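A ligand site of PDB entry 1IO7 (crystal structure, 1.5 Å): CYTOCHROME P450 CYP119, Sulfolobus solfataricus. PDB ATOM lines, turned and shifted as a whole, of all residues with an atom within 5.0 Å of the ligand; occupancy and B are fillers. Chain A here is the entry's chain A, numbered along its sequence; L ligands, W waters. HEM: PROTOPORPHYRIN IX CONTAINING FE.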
ATOM      1  N   LEU A  33     -29.971 -35.277 -15.914  1.00  0.00           N
ATOM      2  CA  LEU A  33     -30.503 -34.422 -14.861  1.00  0.00           C
ATOM      3  C   LEU A  33     -32.015 -34.340 -14.833  1.00  0.00           C
ATOM      4  O   LEU A  33     -32.618 -34.307 -13.770  1.00  0.00           O
ATOM      5  CB  LEU A  33     -29.913 -33.016 -14.995  1.00  0.00           C
ATOM      6  CG  LEU A  33     -28.409 -32.894 -14.707  1.00  0.00           C
ATOM      7  CD1 LEU A  33     -27.945 -31.473 -15.019  1.00  0.00           C
ATOM      8  CD2 LEU A  33     -28.130 -33.249 -13.245  1.00  0.00           C
ATOM      9  N   MET A  68     -33.620 -32.368   0.713  1.00  0.00           N
ATOM     10  CA  MET A  68     -34.266 -32.474  -0.586  1.00  0.00           C
ATOM     11  C   MET A  68     -33.259 -32.815  -1.689  1.00  0.00           C
ATOM     12  O   MET A  68     -33.633 -33.381  -2.717  1.00  0.00           O
ATOM     13  CB  MET A  68     -35.007 -31.174  -0.923  1.00  0.00           C
ATOM     14  CG  MET A  68     -34.113 -29.995  -1.187  1.00  0.00           C
ATOM     15  SD  MET A  68     -35.065 -28.537  -1.650  1.00  0.00           S
ATOM     16  CE  MET A  68     -35.617 -27.905  -0.007  1.00  0.00           C
ATOM     17  N   LEU A  69     -31.986 -32.487  -1.481  1.00  0.00           N
ATOM     18  CA  LEU A  69     -30.946 -32.763  -2.472  1.00  0.00           C
ATOM     19  C   LEU A  69     -30.720 -34.265  -2.699  1.00  0.00           C
ATOM     20  O   LEU A  69     -30.403 -34.676  -3.814  1.00  0.00           O
ATOM     21  CB  LEU A  69     -29.617 -32.129  -2.045  1.00  0.00           C
ATOM     22  CG  LEU A  69     -28.828 -31.233  -3.004  1.00  0.00           C
ATOM     23  CD1 LEU A  69     -27.377 -31.290  -2.560  1.00  0.00           C
ATOM     24  CD2 LEU A  69     -28.973 -31.674  -4.453  1.00  0.00           C
ATOM     25  N   HIS A  76     -39.177 -35.597  -2.634  1.00  0.00           N
ATOM     26  CA  HIS A  76     -38.477 -34.372  -3.026  1.00  0.00           C
ATOM     27  C   HIS A  76     -39.389 -33.179  -3.196  1.00  0.00           C
ATOM     28  O   HIS A  76     -39.067 -32.074  -2.738  1.00  0.00           O
ATOM     29  CB  HIS A  76     -37.703 -34.553  -4.327  1.00  0.00           C
ATOM     30  CG  HIS A  76     -37.178 -33.268  -4.884  1.00  0.00           C
ATOM     31  ND1 HIS A  76     -37.870 -32.532  -5.831  1.00  0.00           N
ATOM     32  CD2 HIS A  76     -36.064 -32.556  -4.594  1.00  0.00           C
ATOM     33  CE1 HIS A  76     -37.201 -31.415  -6.090  1.00  0.00           C
ATOM     34  NE2 HIS A  76     -36.102 -31.405  -5.349  1.00  0.00           N
ATOM     35  N   ARG A  80     -39.391 -29.715  -1.061  1.00  0.00           N
ATOM     36  CA  ARG A  80     -39.123 -28.458  -1.725  1.00  0.00           C
ATOM     37  C   ARG A  80     -40.276 -27.461  -1.705  1.00  0.00           C
ATOM     38  O   ARG A  80     -40.043 -26.260  -1.626  1.00  0.00           O
ATOM     39  CB  ARG A  80     -38.675 -28.724  -3.173  1.00  0.00           C
ATOM     40  CG  ARG A  80     -38.350 -27.439  -3.918  1.00  0.00           C
ATOM     41  CD  ARG A  80     -37.310 -27.646  -4.971  1.00  0.00           C
ATOM     42  NE  ARG A  80     -37.145 -26.414  -5.745  1.00  0.00           N
ATOM     43  CZ  ARG A  80     -36.096 -26.155  -6.510  1.00  0.00           C
ATOM     44  NH1 ARG A  80     -35.120 -27.047  -6.614  1.00  0.00           N
ATOM     45  NH2 ARG A  80     -36.026 -25.007  -7.179  1.00  0.00           N
ATOM     46  N   PHE A  87     -37.143 -17.381  -2.313  1.00  0.00           N
ATOM     47  CA  PHE A  87     -36.393 -16.399  -3.088  1.00  0.00           C
ATOM     48  C   PHE A  87     -37.228 -15.882  -4.261  1.00  0.00           C
ATOM     49  O   PHE A  87     -36.723 -15.695  -5.360  1.00  0.00           O
ATOM     50  CB  PHE A  87     -35.090 -17.023  -3.595  1.00  0.00           C
ATOM     51  CG  PHE A  87     -34.240 -17.627  -2.508  1.00  0.00           C
ATOM     52  CD1 PHE A  87     -33.680 -18.885  -2.661  1.00  0.00           C
ATOM     53  CD2 PHE A  87     -34.021 -16.939  -1.331  1.00  0.00           C
ATOM     54  CE1 PHE A  87     -32.928 -19.451  -1.648  1.00  0.00           C
ATOM     55  CE2 PHE A  87     -33.261 -17.507  -0.295  1.00  0.00           C
ATOM     56  CZ  PHE A  87     -32.711 -18.761  -0.457  1.00  0.00           C
ATOM     57  N   ILE A 130     -27.797 -14.856   3.740  1.00  0.00           N
ATOM     58  CA  ILE A 130     -28.574 -16.024   4.168  1.00  0.00           C
ATOM     59  C   ILE A 130     -28.985 -15.918   5.662  1.00  0.00           C
ATOM     60  O   ILE A 130     -30.080 -16.329   6.028  1.00  0.00           O
ATOM     61  CB  ILE A 130     -27.792 -17.353   3.885  1.00  0.00           C
ATOM     62  CG1 ILE A 130     -28.770 -18.534   3.807  1.00  0.00           C
ATOM     63  CG2 ILE A 130     -26.718 -17.592   4.950  1.00  0.00           C
ATOM     64  CD1 ILE A 130     -29.871 -18.357   2.761  1.00  0.00           C
ATOM     65  N   PHE A 153     -21.445 -30.844  -1.900  1.00  0.00           N
ATOM     66  CA  PHE A 153     -20.643 -30.999  -3.127  1.00  0.00           C
ATOM     67  C   PHE A 153     -19.212 -31.462  -2.814  1.00  0.00           C
ATOM     68  O   PHE A 153     -18.554 -32.074  -3.649  1.00  0.00           O
ATOM     69  CB  PHE A 153     -20.559 -29.673  -3.900  1.00  0.00           C
ATOM     70  CG  PHE A 153     -21.880 -29.166  -4.367  1.00  0.00           C
ATOM     71  CD1 PHE A 153     -22.319 -27.906  -4.004  1.00  0.00           C
ATOM     72  CD2 PHE A 153     -22.708 -29.949  -5.168  1.00  0.00           C
ATOM     73  CE1 PHE A 153     -23.553 -27.430  -4.436  1.00  0.00           C
ATOM     74  CE2 PHE A 153     -23.953 -29.480  -5.601  1.00  0.00           C
ATOM     75  CZ  PHE A 153     -24.365 -28.224  -5.226  1.00  0.00           C
ATOM     76  N   LEU A 205     -29.085 -27.354   5.161  1.00  0.00           N
ATOM     77  CA  LEU A 205     -28.991 -27.205   3.702  1.00  0.00           C
ATOM     78  C   LEU A 205     -29.201 -25.743   3.292  1.00  0.00           C
ATOM     79  O   LEU A 205     -28.412 -25.183   2.550  1.00  0.00           O
ATOM     80  CB  LEU A 205     -30.033 -28.085   2.979  1.00  0.00           C
ATOM     81  CG  LEU A 205     -30.184 -27.897   1.456  1.00  0.00           C
ATOM     82  CD1 LEU A 205     -28.936 -28.380   0.737  1.00  0.00           C
ATOM     83  CD2 LEU A 205     -31.390 -28.664   0.963  1.00  0.00           C
ATOM     84  N   LEU A 206     -30.269 -25.136   3.799  1.00  0.00           N
ATOM     85  CA  LEU A 206     -30.554 -23.750   3.474  1.00  0.00           C
ATOM     86  C   LEU A 206     -29.433 -22.833   3.958  1.00  0.00           C
ATOM     87  O   LEU A 206     -29.085 -21.854   3.299  1.00  0.00           O
ATOM     88  CB  LEU A 206     -31.869 -23.322   4.109  1.00  0.00           C
ATOM     89  CG  LEU A 206     -33.120 -24.017   3.538  1.00  0.00           C
ATOM     90  CD1 LEU A 206     -34.333 -23.473   4.262  1.00  0.00           C
ATOM     91  CD2 LEU A 206     -33.233 -23.773   2.036  1.00  0.00           C
ATOM     92  N   ALA A 209     -25.843 -24.454   1.770  1.00  0.00           N
ATOM     93  CA  ALA A 209     -25.842 -24.824   0.358  1.00  0.00           C
ATOM     94  C   ALA A 209     -25.312 -23.766  -0.592  1.00  0.00           C
ATOM     95  O   ALA A 209     -24.728 -24.100  -1.628  1.00  0.00           O
ATOM     96  CB  ALA A 209     -27.233 -25.268  -0.079  1.00  0.00           C
ATOM     97  N   GLY A 210     -25.486 -22.488  -0.271  1.00  0.00           N
ATOM     98  CA  GLY A 210     -25.012 -21.486  -1.201  1.00  0.00           C
ATOM     99  C   GLY A 210     -23.833 -20.618  -0.815  1.00  0.00           C
ATOM    100  O   GLY A 210     -23.482 -19.697  -1.559  1.00  0.00           O
ATOM    101  N   THR A 213     -20.419 -21.818  -2.925  1.00  0.00           N
ATOM    102  CA  THR A 213     -20.753 -21.688  -4.348  1.00  0.00           C
ATOM    103  C   THR A 213     -20.922 -20.236  -4.764  1.00  0.00           C
ATOM    104  O   THR A 213     -20.385 -19.827  -5.805  1.00  0.00           O
ATOM    105  CB  THR A 213     -22.054 -22.445  -4.708  1.00  0.00           C
ATOM    106  OG1 THR A 213     -23.115 -22.052  -3.825  1.00  0.00           O
ATOM    107  CG2 THR A 213     -21.827 -23.967  -4.648  1.00  0.00           C
ATOM    108  N   THR A 214     -21.651 -19.439  -3.984  1.00  0.00           N
ATOM    109  CA  THR A 214     -21.866 -18.039  -4.336  1.00  0.00           C
ATOM    110  C   THR A 214     -20.561 -17.260  -4.226  1.00  0.00           C
ATOM    111  O   THR A 214     -20.262 -16.368  -5.040  1.00  0.00           O
ATOM    112  CB  THR A 214     -22.935 -17.387  -3.436  1.00  0.00           C
ATOM    113  OG1 THR A 214     -24.178 -18.071  -3.622  1.00  0.00           O
ATOM    114  CG2 THR A 214     -23.127 -15.929  -3.814  1.00  0.00           C
ATOM    115  N   LEU A 217     -18.685 -17.880  -7.317  1.00  0.00           N
ATOM    116  CA  LEU A 217     -19.218 -17.155  -8.467  1.00  0.00           C
ATOM    117  C   LEU A 217     -18.593 -15.748  -8.501  1.00  0.00           C
ATOM    118  O   LEU A 217     -18.099 -15.290  -9.534  1.00  0.00           O
ATOM    119  CB  LEU A 217     -20.753 -17.051  -8.345  1.00  0.00           C
ATOM    120  CG  LEU A 217     -21.436 -16.066  -9.307  1.00  0.00           C
ATOM    121  CD1 LEU A 217     -20.974 -16.317 -10.733  1.00  0.00           C
ATOM    122  CD2 LEU A 217     -22.943 -16.236  -9.218  1.00  0.00           C
ATOM    123  N   LEU A 248     -20.677 -17.938 -14.989  1.00  0.00           N
ATOM    124  CA  LEU A 248     -21.266 -19.182 -14.530  1.00  0.00           C
ATOM    125  C   LEU A 248     -21.006 -20.295 -15.550  1.00  0.00           C
ATOM    126  O   LEU A 248     -20.678 -21.423 -15.197  1.00  0.00           O
ATOM    127  CB  LEU A 248     -22.783 -19.024 -14.347  1.00  0.00           C
ATOM    128  CG  LEU A 248     -23.248 -18.445 -13.022  1.00  0.00           C
ATOM    129  CD1 LEU A 248     -24.654 -17.898 -13.176  1.00  0.00           C
ATOM    130  CD2 LEU A 248     -23.155 -19.535 -11.948  1.00  0.00           C
ATOM    131  N   PRO A 253     -18.986 -22.734 -10.518  1.00  0.00           N
ATOM    132  CA  PRO A 253     -18.601 -22.997  -9.116  1.00  0.00           C
ATOM    133  C   PRO A 253     -18.683 -24.502  -8.780  1.00  0.00           C
ATOM    134  O   PRO A 253     -17.951 -24.998  -7.913  1.00  0.00           O
ATOM    135  CB  PRO A 253     -19.586 -22.156  -8.316  1.00  0.00           C
ATOM    136  CG  PRO A 253     -20.008 -21.065  -9.254  1.00  0.00           C
ATOM    137  CD  PRO A 253     -20.046 -21.721 -10.622  1.00  0.00           C
ATOM    138  N   VAL A 254     -19.588 -25.213  -9.446  1.00  0.00           N
ATOM    139  CA  VAL A 254     -19.755 -26.653  -9.252  1.00  0.00           C
ATOM    140  C   VAL A 254     -19.467 -27.333 -10.601  1.00  0.00           C
ATOM    141  O   VAL A 254     -20.203 -27.155 -11.589  1.00  0.00           O
ATOM    142  CB  VAL A 254     -21.190 -27.018  -8.787  1.00  0.00           C
ATOM    143  CG1 VAL A 254     -21.299 -28.526  -8.623  1.00  0.00           C
ATOM    144  CG2 VAL A 254     -21.497 -26.308  -7.460  1.00  0.00           C
ATOM    145  N   THR A 257     -21.967 -33.157 -10.957  1.00  0.00           N
ATOM    146  CA  THR A 257     -22.904 -33.690  -9.978  1.00  0.00           C
ATOM    147  C   THR A 257     -22.999 -35.199 -10.218  1.00  0.00           C
ATOM    148  O   THR A 257     -22.429 -35.732 -11.175  1.00  0.00           O
ATOM    149  CB  THR A 257     -24.308 -33.028 -10.076  1.00  0.00           C
ATOM    150  OG1 THR A 257     -25.109 -33.473  -8.970  1.00  0.00           O
ATOM    151  CG2 THR A 257     -25.002 -33.388 -11.375  1.00  0.00           C
ATOM    152  N   VAL A 258     -23.706 -35.904  -9.345  1.00  0.00           N
ATOM    153  CA  VAL A 258     -23.809 -37.352  -9.472  1.00  0.00           C
ATOM    154  C   VAL A 258     -25.244 -37.840  -9.374  1.00  0.00           C
ATOM    155  O   VAL A 258     -26.095 -37.196  -8.767  1.00  0.00           O
ATOM    156  CB  VAL A 258     -23.002 -38.082  -8.382  1.00  0.00           C
ATOM    157  CG1 VAL A 258     -23.444 -37.590  -7.025  1.00  0.00           C
ATOM    158  CG2 VAL A 258     -23.198 -39.584  -8.481  1.00  0.00           C
ATOM    159  N   ARG A 259     -25.477 -38.993 -10.005  1.00  0.00           N
ATOM    160  CA  ARG A 259     -26.777 -39.653 -10.008  1.00  0.00           C
ATOM    161  C   ARG A 259     -26.472 -41.150  -9.960  1.00  0.00           C
ATOM    162  O   ARG A 259     -25.334 -41.581 -10.170  1.00  0.00           O
ATOM    163  CB  ARG A 259     -27.558 -39.340 -11.293  1.00  0.00           C
ATOM    164  CG  ARG A 259     -28.045 -37.893 -11.439  1.00  0.00           C
ATOM    165  CD  ARG A 259     -28.932 -37.457 -10.285  1.00  0.00           C
ATOM    166  NE  ARG A 259     -29.573 -36.155 -10.495  1.00  0.00           N
ATOM    167  CZ  ARG A 259     -29.098 -34.993 -10.062  1.00  0.00           C
ATOM    168  NH1 ARG A 259     -27.948 -34.926  -9.378  1.00  0.00           N
ATOM    169  NH2 ARG A 259     -29.809 -33.878 -10.249  1.00  0.00           N
ATOM    170  N   ILE A 282     -20.977 -30.968 -15.511  1.00  0.00           N
ATOM    171  CA  ILE A 282     -21.581 -29.682 -15.828  1.00  0.00           C
ATOM    172  C   ILE A 282     -20.574 -28.777 -16.561  1.00  0.00           C
ATOM    173  O   ILE A 282     -20.927 -28.106 -17.539  1.00  0.00           O
ATOM    174  CB  ILE A 282     -22.022 -28.960 -14.535  1.00  0.00           C
ATOM    175  CG1 ILE A 282     -23.370 -29.502 -14.071  1.00  0.00           C
ATOM    176  CG2 ILE A 282     -22.057 -27.446 -14.777  1.00  0.00           C
ATOM    177  CD1 ILE A 282     -23.639 -29.199 -12.611  1.00  0.00           C
ATOM    178  N   SER A 309     -24.978 -24.751 -14.823  1.00  0.00           N
ATOM    179  CA  SER A 309     -24.245 -24.503 -13.581  1.00  0.00           C
ATOM    180  C   SER A 309     -25.090 -24.578 -12.320  1.00  0.00           C
ATOM    181  O   SER A 309     -24.558 -24.785 -11.212  1.00  0.00           O
ATOM    182  CB  SER A 309     -23.544 -23.149 -13.681  1.00  0.00           C
ATOM    183  OG  SER A 309     -22.647 -23.218 -14.780  1.00  0.00           O
ATOM    184  N   PHE A 310     -26.405 -24.400 -12.467  1.00  0.00           N
ATOM    185  CA  PHE A 310     -27.326 -24.488 -11.341  1.00  0.00           C
ATOM    186  C   PHE A 310     -28.095 -25.816 -11.476  1.00  0.00           C
ATOM    187  O   PHE A 310     -29.061 -26.055 -10.749  1.00  0.00           O
ATOM    188  CB  PHE A 310     -28.309 -23.343 -11.379  1.00  0.00           C
ATOM    189  CG  PHE A 310     -27.744 -22.025 -10.960  1.00  0.00           C
ATOM    190  CD1 PHE A 310     -27.760 -20.931 -11.840  1.00  0.00           C
ATOM    191  CD2 PHE A 310     -27.232 -21.850  -9.667  1.00  0.00           C
ATOM    192  CE1 PHE A 310     -27.289 -19.684 -11.449  1.00  0.00           C
ATOM    193  CE2 PHE A 310     -26.752 -20.593  -9.261  1.00  0.00           C
ATOM    194  CZ  PHE A 310     -26.782 -19.501 -10.158  1.00  0.00           C
ATOM    195  N   GLY A 311     -27.661 -26.655 -12.412  1.00  0.00           N
ATOM    196  CA  GLY A 311     -28.334 -27.915 -12.626  1.00  0.00           C
ATOM    197  C   GLY A 311     -29.444 -27.776 -13.653  1.00  0.00           C
ATOM    198  O   GLY A 311     -29.424 -26.852 -14.479  1.00  0.00           O
ATOM    199  N   ILE A 314     -35.875 -31.078 -11.749  1.00  0.00           N
ATOM    200  CA  ILE A 314     -36.480 -30.844 -10.441  1.00  0.00           C
ATOM    201  C   ILE A 314     -35.551 -30.341  -9.332  1.00  0.00           C
ATOM    202  O   ILE A 314     -36.009 -29.733  -8.373  1.00  0.00           O
ATOM    203  CB  ILE A 314     -37.202 -32.100  -9.931  1.00  0.00           C
ATOM    204  CG1 ILE A 314     -36.189 -33.221  -9.695  1.00  0.00           C
ATOM    205  CG2 ILE A 314     -38.273 -32.533 -10.930  1.00  0.00           C
ATOM    206  CD1 ILE A 314     -36.780 -34.380  -8.966  1.00  0.00           C
ATOM    207  N   HIS A 315     -34.236 -30.602  -9.441  1.00  0.00           N
ATOM    208  CA  HIS A 315     -33.292 -30.149  -8.417  1.00  0.00           C
ATOM    209  C   HIS A 315     -32.603 -28.824  -8.776  1.00  0.00           C
ATOM    210  O   HIS A 315     -31.671 -28.382  -8.079  1.00  0.00           O
ATOM    211  CB  HIS A 315     -32.233 -31.205  -8.147  1.00  0.00           C
ATOM    212  CG  HIS A 315     -32.769 -32.455  -7.525  1.00  0.00           C
ATOM    213  ND1 HIS A 315     -33.009 -32.557  -6.172  1.00  0.00           N
ATOM    214  CD2 HIS A 315     -33.073 -33.666  -8.058  1.00  0.00           C
ATOM    215  CE1 HIS A 315     -33.436 -33.779  -5.898  1.00  0.00           C
ATOM    216  NE2 HIS A 315     -33.481 -34.474  -7.029  1.00  0.00           N
ATOM    217  N   LEU A 316     -33.058 -28.205  -9.874  1.00  0.00           N
ATOM    218  CA  LEU A 316     -32.531 -26.912 -10.315  1.00  0.00           C
ATOM    219  C   LEU A 316     -32.365 -26.067  -9.062  1.00  0.00           C
ATOM    220  O   LEU A 316     -33.330 -25.822  -8.328  1.00  0.00           O
ATOM    221  CB  LEU A 316     -33.527 -26.247 -11.271  1.00  0.00           C
ATOM    222  CG  LEU A 316     -33.111 -25.394 -12.472  1.00  0.00           C
ATOM    223  CD1 LEU A 316     -34.119 -24.272 -12.670  1.00  0.00           C
ATOM    224  CD2 LEU A 316     -31.742 -24.840 -12.302  1.00  0.00           C
ATOM    225  N   CYS A 317     -31.144 -25.593  -8.826  1.00  0.00           N
ATOM    226  CA  CYS A 317     -30.826 -24.812  -7.637  1.00  0.00           C
ATOM    227  C   CYS A 317     -31.928 -23.881  -7.126  1.00  0.00           C
ATOM    228  O   CYS A 317     -32.384 -22.989  -7.852  1.00  0.00           O
ATOM    229  CB  CYS A 317     -29.540 -24.005  -7.876  1.00  0.00           C
ATOM    230  SG  CYS A 317     -29.015 -23.028  -6.433  1.00  0.00           S
ATOM    231  N   LEU A 318     -32.335 -24.101  -5.888  1.00  0.00           N
ATOM    232  CA  LEU A 318     -33.374 -23.302  -5.244  1.00  0.00           C
ATOM    233  C   LEU A 318     -32.883 -21.866  -5.024  1.00  0.00           C
ATOM    234  O   LEU A 318     -33.681 -20.920  -5.027  1.00  0.00           O
ATOM    235  CB  LEU A 318     -33.725 -23.918  -3.878  1.00  0.00           C
ATOM    236  CG  LEU A 318     -35.124 -23.792  -3.241  1.00  0.00           C
ATOM    237  CD1 LEU A 318     -34.947 -23.541  -1.751  1.00  0.00           C
ATOM    238  CD2 LEU A 318     -35.960 -22.710  -3.874  1.00  0.00           C
ATOM    239  N   GLY A 319     -31.579 -21.719  -4.833  1.00  0.00           N
ATOM    240  CA  GLY A 319     -31.024 -20.405  -4.583  1.00  0.00           C
ATOM    241  C   GLY A 319     -30.543 -19.621  -5.791  1.00  0.00           C
ATOM    242  O   GLY A 319     -29.985 -18.538  -5.628  1.00  0.00           O
ATOM    243  N   ALA A 320     -30.755 -20.153  -6.998  1.00  0.00           N
ATOM    244  CA  ALA A 320     -30.295 -19.500  -8.227  1.00  0.00           C
ATOM    245  C   ALA A 320     -30.625 -17.998  -8.331  1.00  0.00           C
ATOM    246  O   ALA A 320     -29.736 -17.184  -8.613  1.00  0.00           O
ATOM    247  CB  ALA A 320     -30.814 -20.248  -9.435  1.00  0.00           C
ATOM    248  N   LEU A 322     -31.250 -15.836  -6.002  1.00  0.00           N
ATOM    249  CA  LEU A 322     -30.532 -15.138  -4.925  1.00  0.00           C
ATOM    250  C   LEU A 322     -29.051 -15.027  -5.256  1.00  0.00           C
ATOM    251  O   LEU A 322     -28.476 -13.950  -5.156  1.00  0.00           O
ATOM    252  CB  LEU A 322     -30.688 -15.893  -3.597  1.00  0.00           C
ATOM    253  CG  LEU A 322     -30.782 -15.157  -2.244  1.00  0.00           C
ATOM    254  CD1 LEU A 322     -30.081 -16.008  -1.154  1.00  0.00           C
ATOM    255  CD2 LEU A 322     -30.176 -13.767  -2.337  1.00  0.00           C
ATOM    256  N   ALA A 323     -28.452 -16.140  -5.656  1.00  0.00           N
ATOM    257  CA  ALA A 323     -27.034 -16.149  -6.002  1.00  0.00           C
ATOM    258  C   ALA A 323     -26.787 -15.158  -7.139  1.00  0.00           C
ATOM    259  O   ALA A 323     -25.819 -14.393  -7.109  1.00  0.00           O
ATOM    260  CB  ALA A 323     -26.608 -17.532  -6.421  1.00  0.00           C
HETATM  261  CHA HEM L   1     -29.076 -27.283  -5.649  1.00  0.00           C
HETATM  262  CHB HEM L   1     -25.366 -24.892  -7.659  1.00  0.00           C
HETATM  263  CHC HEM L   1     -26.256 -21.096  -4.789  1.00  0.00           C
HETATM  264  CHD HEM L   1     -29.573 -23.729  -2.367  1.00  0.00           C
HETATM  265  C1A HEM L   1     -28.053 -26.927  -6.492  1.00  0.00           C
HETATM  266  C2A HEM L   1     -27.594 -27.730  -7.632  1.00  0.00           C
HETATM  267  C3A HEM L   1     -26.496 -27.070  -8.130  1.00  0.00           C
HETATM  268  C4A HEM L   1     -26.319 -25.878  -7.355  1.00  0.00           C
HETATM  269  CMA HEM L   1     -25.588 -27.566  -9.242  1.00  0.00           C
HETATM  270  CAA HEM L   1     -28.195 -29.032  -8.176  1.00  0.00           C
HETATM  271  CBA HEM L   1     -27.534 -30.248  -7.561  1.00  0.00           C
HETATM  272  CGA HEM L   1     -28.003 -31.574  -8.157  1.00  0.00           C
HETATM  273  O1A HEM L   1     -28.706 -31.562  -9.201  1.00  0.00           O
HETATM  274  O2A HEM L   1     -27.670 -32.630  -7.597  1.00  0.00           O
HETATM  275  C1B HEM L   1     -25.257 -23.659  -7.019  1.00  0.00           C
HETATM  276  C2B HEM L   1     -24.389 -22.552  -7.531  1.00  0.00           C
HETATM  277  C3B HEM L   1     -24.642 -21.493  -6.683  1.00  0.00           C
HETATM  278  C4B HEM L   1     -25.679 -21.929  -5.736  1.00  0.00           C
HETATM  279  CMB HEM L   1     -23.506 -22.544  -8.811  1.00  0.00           C
HETATM  280  CAB HEM L   1     -24.045 -20.213  -6.667  1.00  0.00           C
HETATM  281  CBB HEM L   1     -23.721 -19.470  -7.817  1.00  0.00           C
HETATM  282  C1C HEM L   1     -27.241 -21.462  -3.894  1.00  0.00           C
HETATM  283  C2C HEM L   1     -27.818 -20.563  -2.885  1.00  0.00           C
HETATM  284  C3C HEM L   1     -28.712 -21.332  -2.152  1.00  0.00           C
HETATM  285  C4C HEM L   1     -28.710 -22.678  -2.755  1.00  0.00           C
HETATM  286  CMC HEM L   1     -27.526 -19.068  -2.731  1.00  0.00           C
HETATM  287  CAC HEM L   1     -29.522 -20.860  -1.098  1.00  0.00           C
HETATM  288  CBC HEM L   1     -29.580 -21.453   0.179  1.00  0.00           C
HETATM  289  C1D HEM L   1     -29.669 -24.967  -3.011  1.00  0.00           C
HETATM  290  C2D HEM L   1     -30.629 -25.988  -2.638  1.00  0.00           C
HETATM  291  C3D HEM L   1     -30.489 -26.998  -3.572  1.00  0.00           C
HETATM  292  C4D HEM L   1     -29.455 -26.570  -4.540  1.00  0.00           C
HETATM  293  CMD HEM L   1     -31.579 -25.915  -1.440  1.00  0.00           C
HETATM  294  CAD HEM L   1     -31.289 -28.284  -3.703  1.00  0.00           C
HETATM  295  CBD HEM L   1     -32.610 -28.083  -4.436  1.00  0.00           C
HETATM  296  CGD HEM L   1     -33.316 -29.395  -4.758  1.00  0.00           C
HETATM  297  O1D HEM L   1     -34.455 -29.359  -5.274  1.00  0.00           O
HETATM  298  O2D HEM L   1     -32.706 -30.459  -4.502  1.00  0.00           O
HETATM  299  NA  HEM L   1     -27.289 -25.769  -6.333  1.00  0.00           N
HETATM  300  NB  HEM L   1     -26.066 -23.238  -5.972  1.00  0.00           N
HETATM  301  NC  HEM L   1     -27.823 -22.748  -3.834  1.00  0.00           N
HETATM  302  ND  HEM L   1     -28.950 -25.332  -4.178  1.00  0.00           N
HETATM  303 FE   HEM L   1     -27.591 -24.227  -5.131  1.00  0.00          FE
HETATM  304  O   HOH W   1     -30.162 -30.331 -11.392  1.00  0.00           O
HETATM  305  O   HOH W   2     -26.976 -27.619  -2.744  1.00  0.00           O
HETATM  306  O   HOH W   3     -25.956 -25.096  -3.819  1.00  0.00           O
HETATM  307  O   HOH W   4     -26.779 -21.079   1.927  1.00  0.00           O
HETATM  308  O   HOH W   5     -25.877 -33.270  -5.695  1.00  0.00           O
HETATM  309  O   HOH W   6     -29.554 -34.176  -6.381  1.00  0.00           O
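An oxygen (O1A) of the ligand lies within salt-bridge range of the guanidinium group (NH2) of Arg 259 (2.8 Å).
An iron atom (FE) of the ligand is bound by the side-chain sulfur (SG) of Cys 317 (2.3 Å).
A ring nitrogen (NE2) of His 76 is in hydrogen-bond range of an oxygen (O1D) of the ligand, 2.6 Å away.
An oxygen (O2A) of the ligand sits at hydrogen-bond distance from the side-chain hydroxyl of Thr 257, 3.0 Å away.
O1D of the ligand lies within salt-bridge range of NH1 of Arg 80.
A ring nitrogen (ND1) of His 315 is in hydrogen-bond range of an oxygen (O2D) of the ligand.
SG of Cys 317 sits close to N of Gly 319, at 3.3 Å.
OG1 of Thr 213 lies within hydrogen-bond range of O of Ala 209, 3.4 Å away.
NE2 of His 76 lies within hydrogen-bond range of ND1 of His 315, 3.4 Å away.
The side-chain hydroxyl of Thr 213 lies close to the backbone carbonyl oxygen of Gly 210 (3.3 Å).
N of Ala 320 sits close to SG of Cys 317, 3.4 Å away.
The side-chain hydroxyl (OG1) of Thr 257 sits at hydrogen-bond distance from the guanidinium group (NH1) of Arg 259, at 3.2 Å.
The side-chain hydroxyl of Thr 214 sits at hydrogen-bond distance from the backbone carbonyl oxygen of Gly 210, at 2.7 Å.
The guanidinium group (NH1) of Arg 80 sits at hydrogen-bond distance from the backbone carbonyl oxygen (O) of Ile 314, at 3.3 Å.
O1D of the ligand lies close to SD of Met 68 (3.8 Å).
The backbone carbonyl oxygen of Ile 314 lies close to an oxygen (O1D) of the ligand.
Merely in contact with the ligand: Leu 206 (3.2 Å), Thr 213 (3.2 Å), Gly 210 (3.4 Å), Ser 309 (3.4 Å), Phe 310 (3.5 Å), Gly 319 (3.5 Å), Leu 69 (3.5 Å), Thr 214 (3.6 Å), Leu 217 (3.6 Å), Ala 209 (3.6 Å), Leu 205 (3.7 Å), Ala 323 (3.7 Å), Phe 153 (3.7 Å), Phe 87 (3.7 Å), Leu 318 (3.8 Å), Pro 253 (3.8 Å) and Gly 311 (3.9 Å).
Hydrophobic or aromatic side chains that line the ligand: Met 68, Leu 69, His 76, Phe 87, Phe 153, Leu 205, Ala 209, Leu 217, Pro 253, Phe 310, His 315, Leu 318 and Ala 323.
Water W5 bridges an oxygen (O2A) of the ligand and the side-chain hydroxyl of Thr 257.
Water W6 lies within hydrogen-bond range of an oxygen (O2A) of the ligand (2.7 Å), the backbone carbonyl oxygen (O) of Leu 69 (2.7 Å) and the guanidinium group (NH1) of Arg 259 (3.5 Å).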
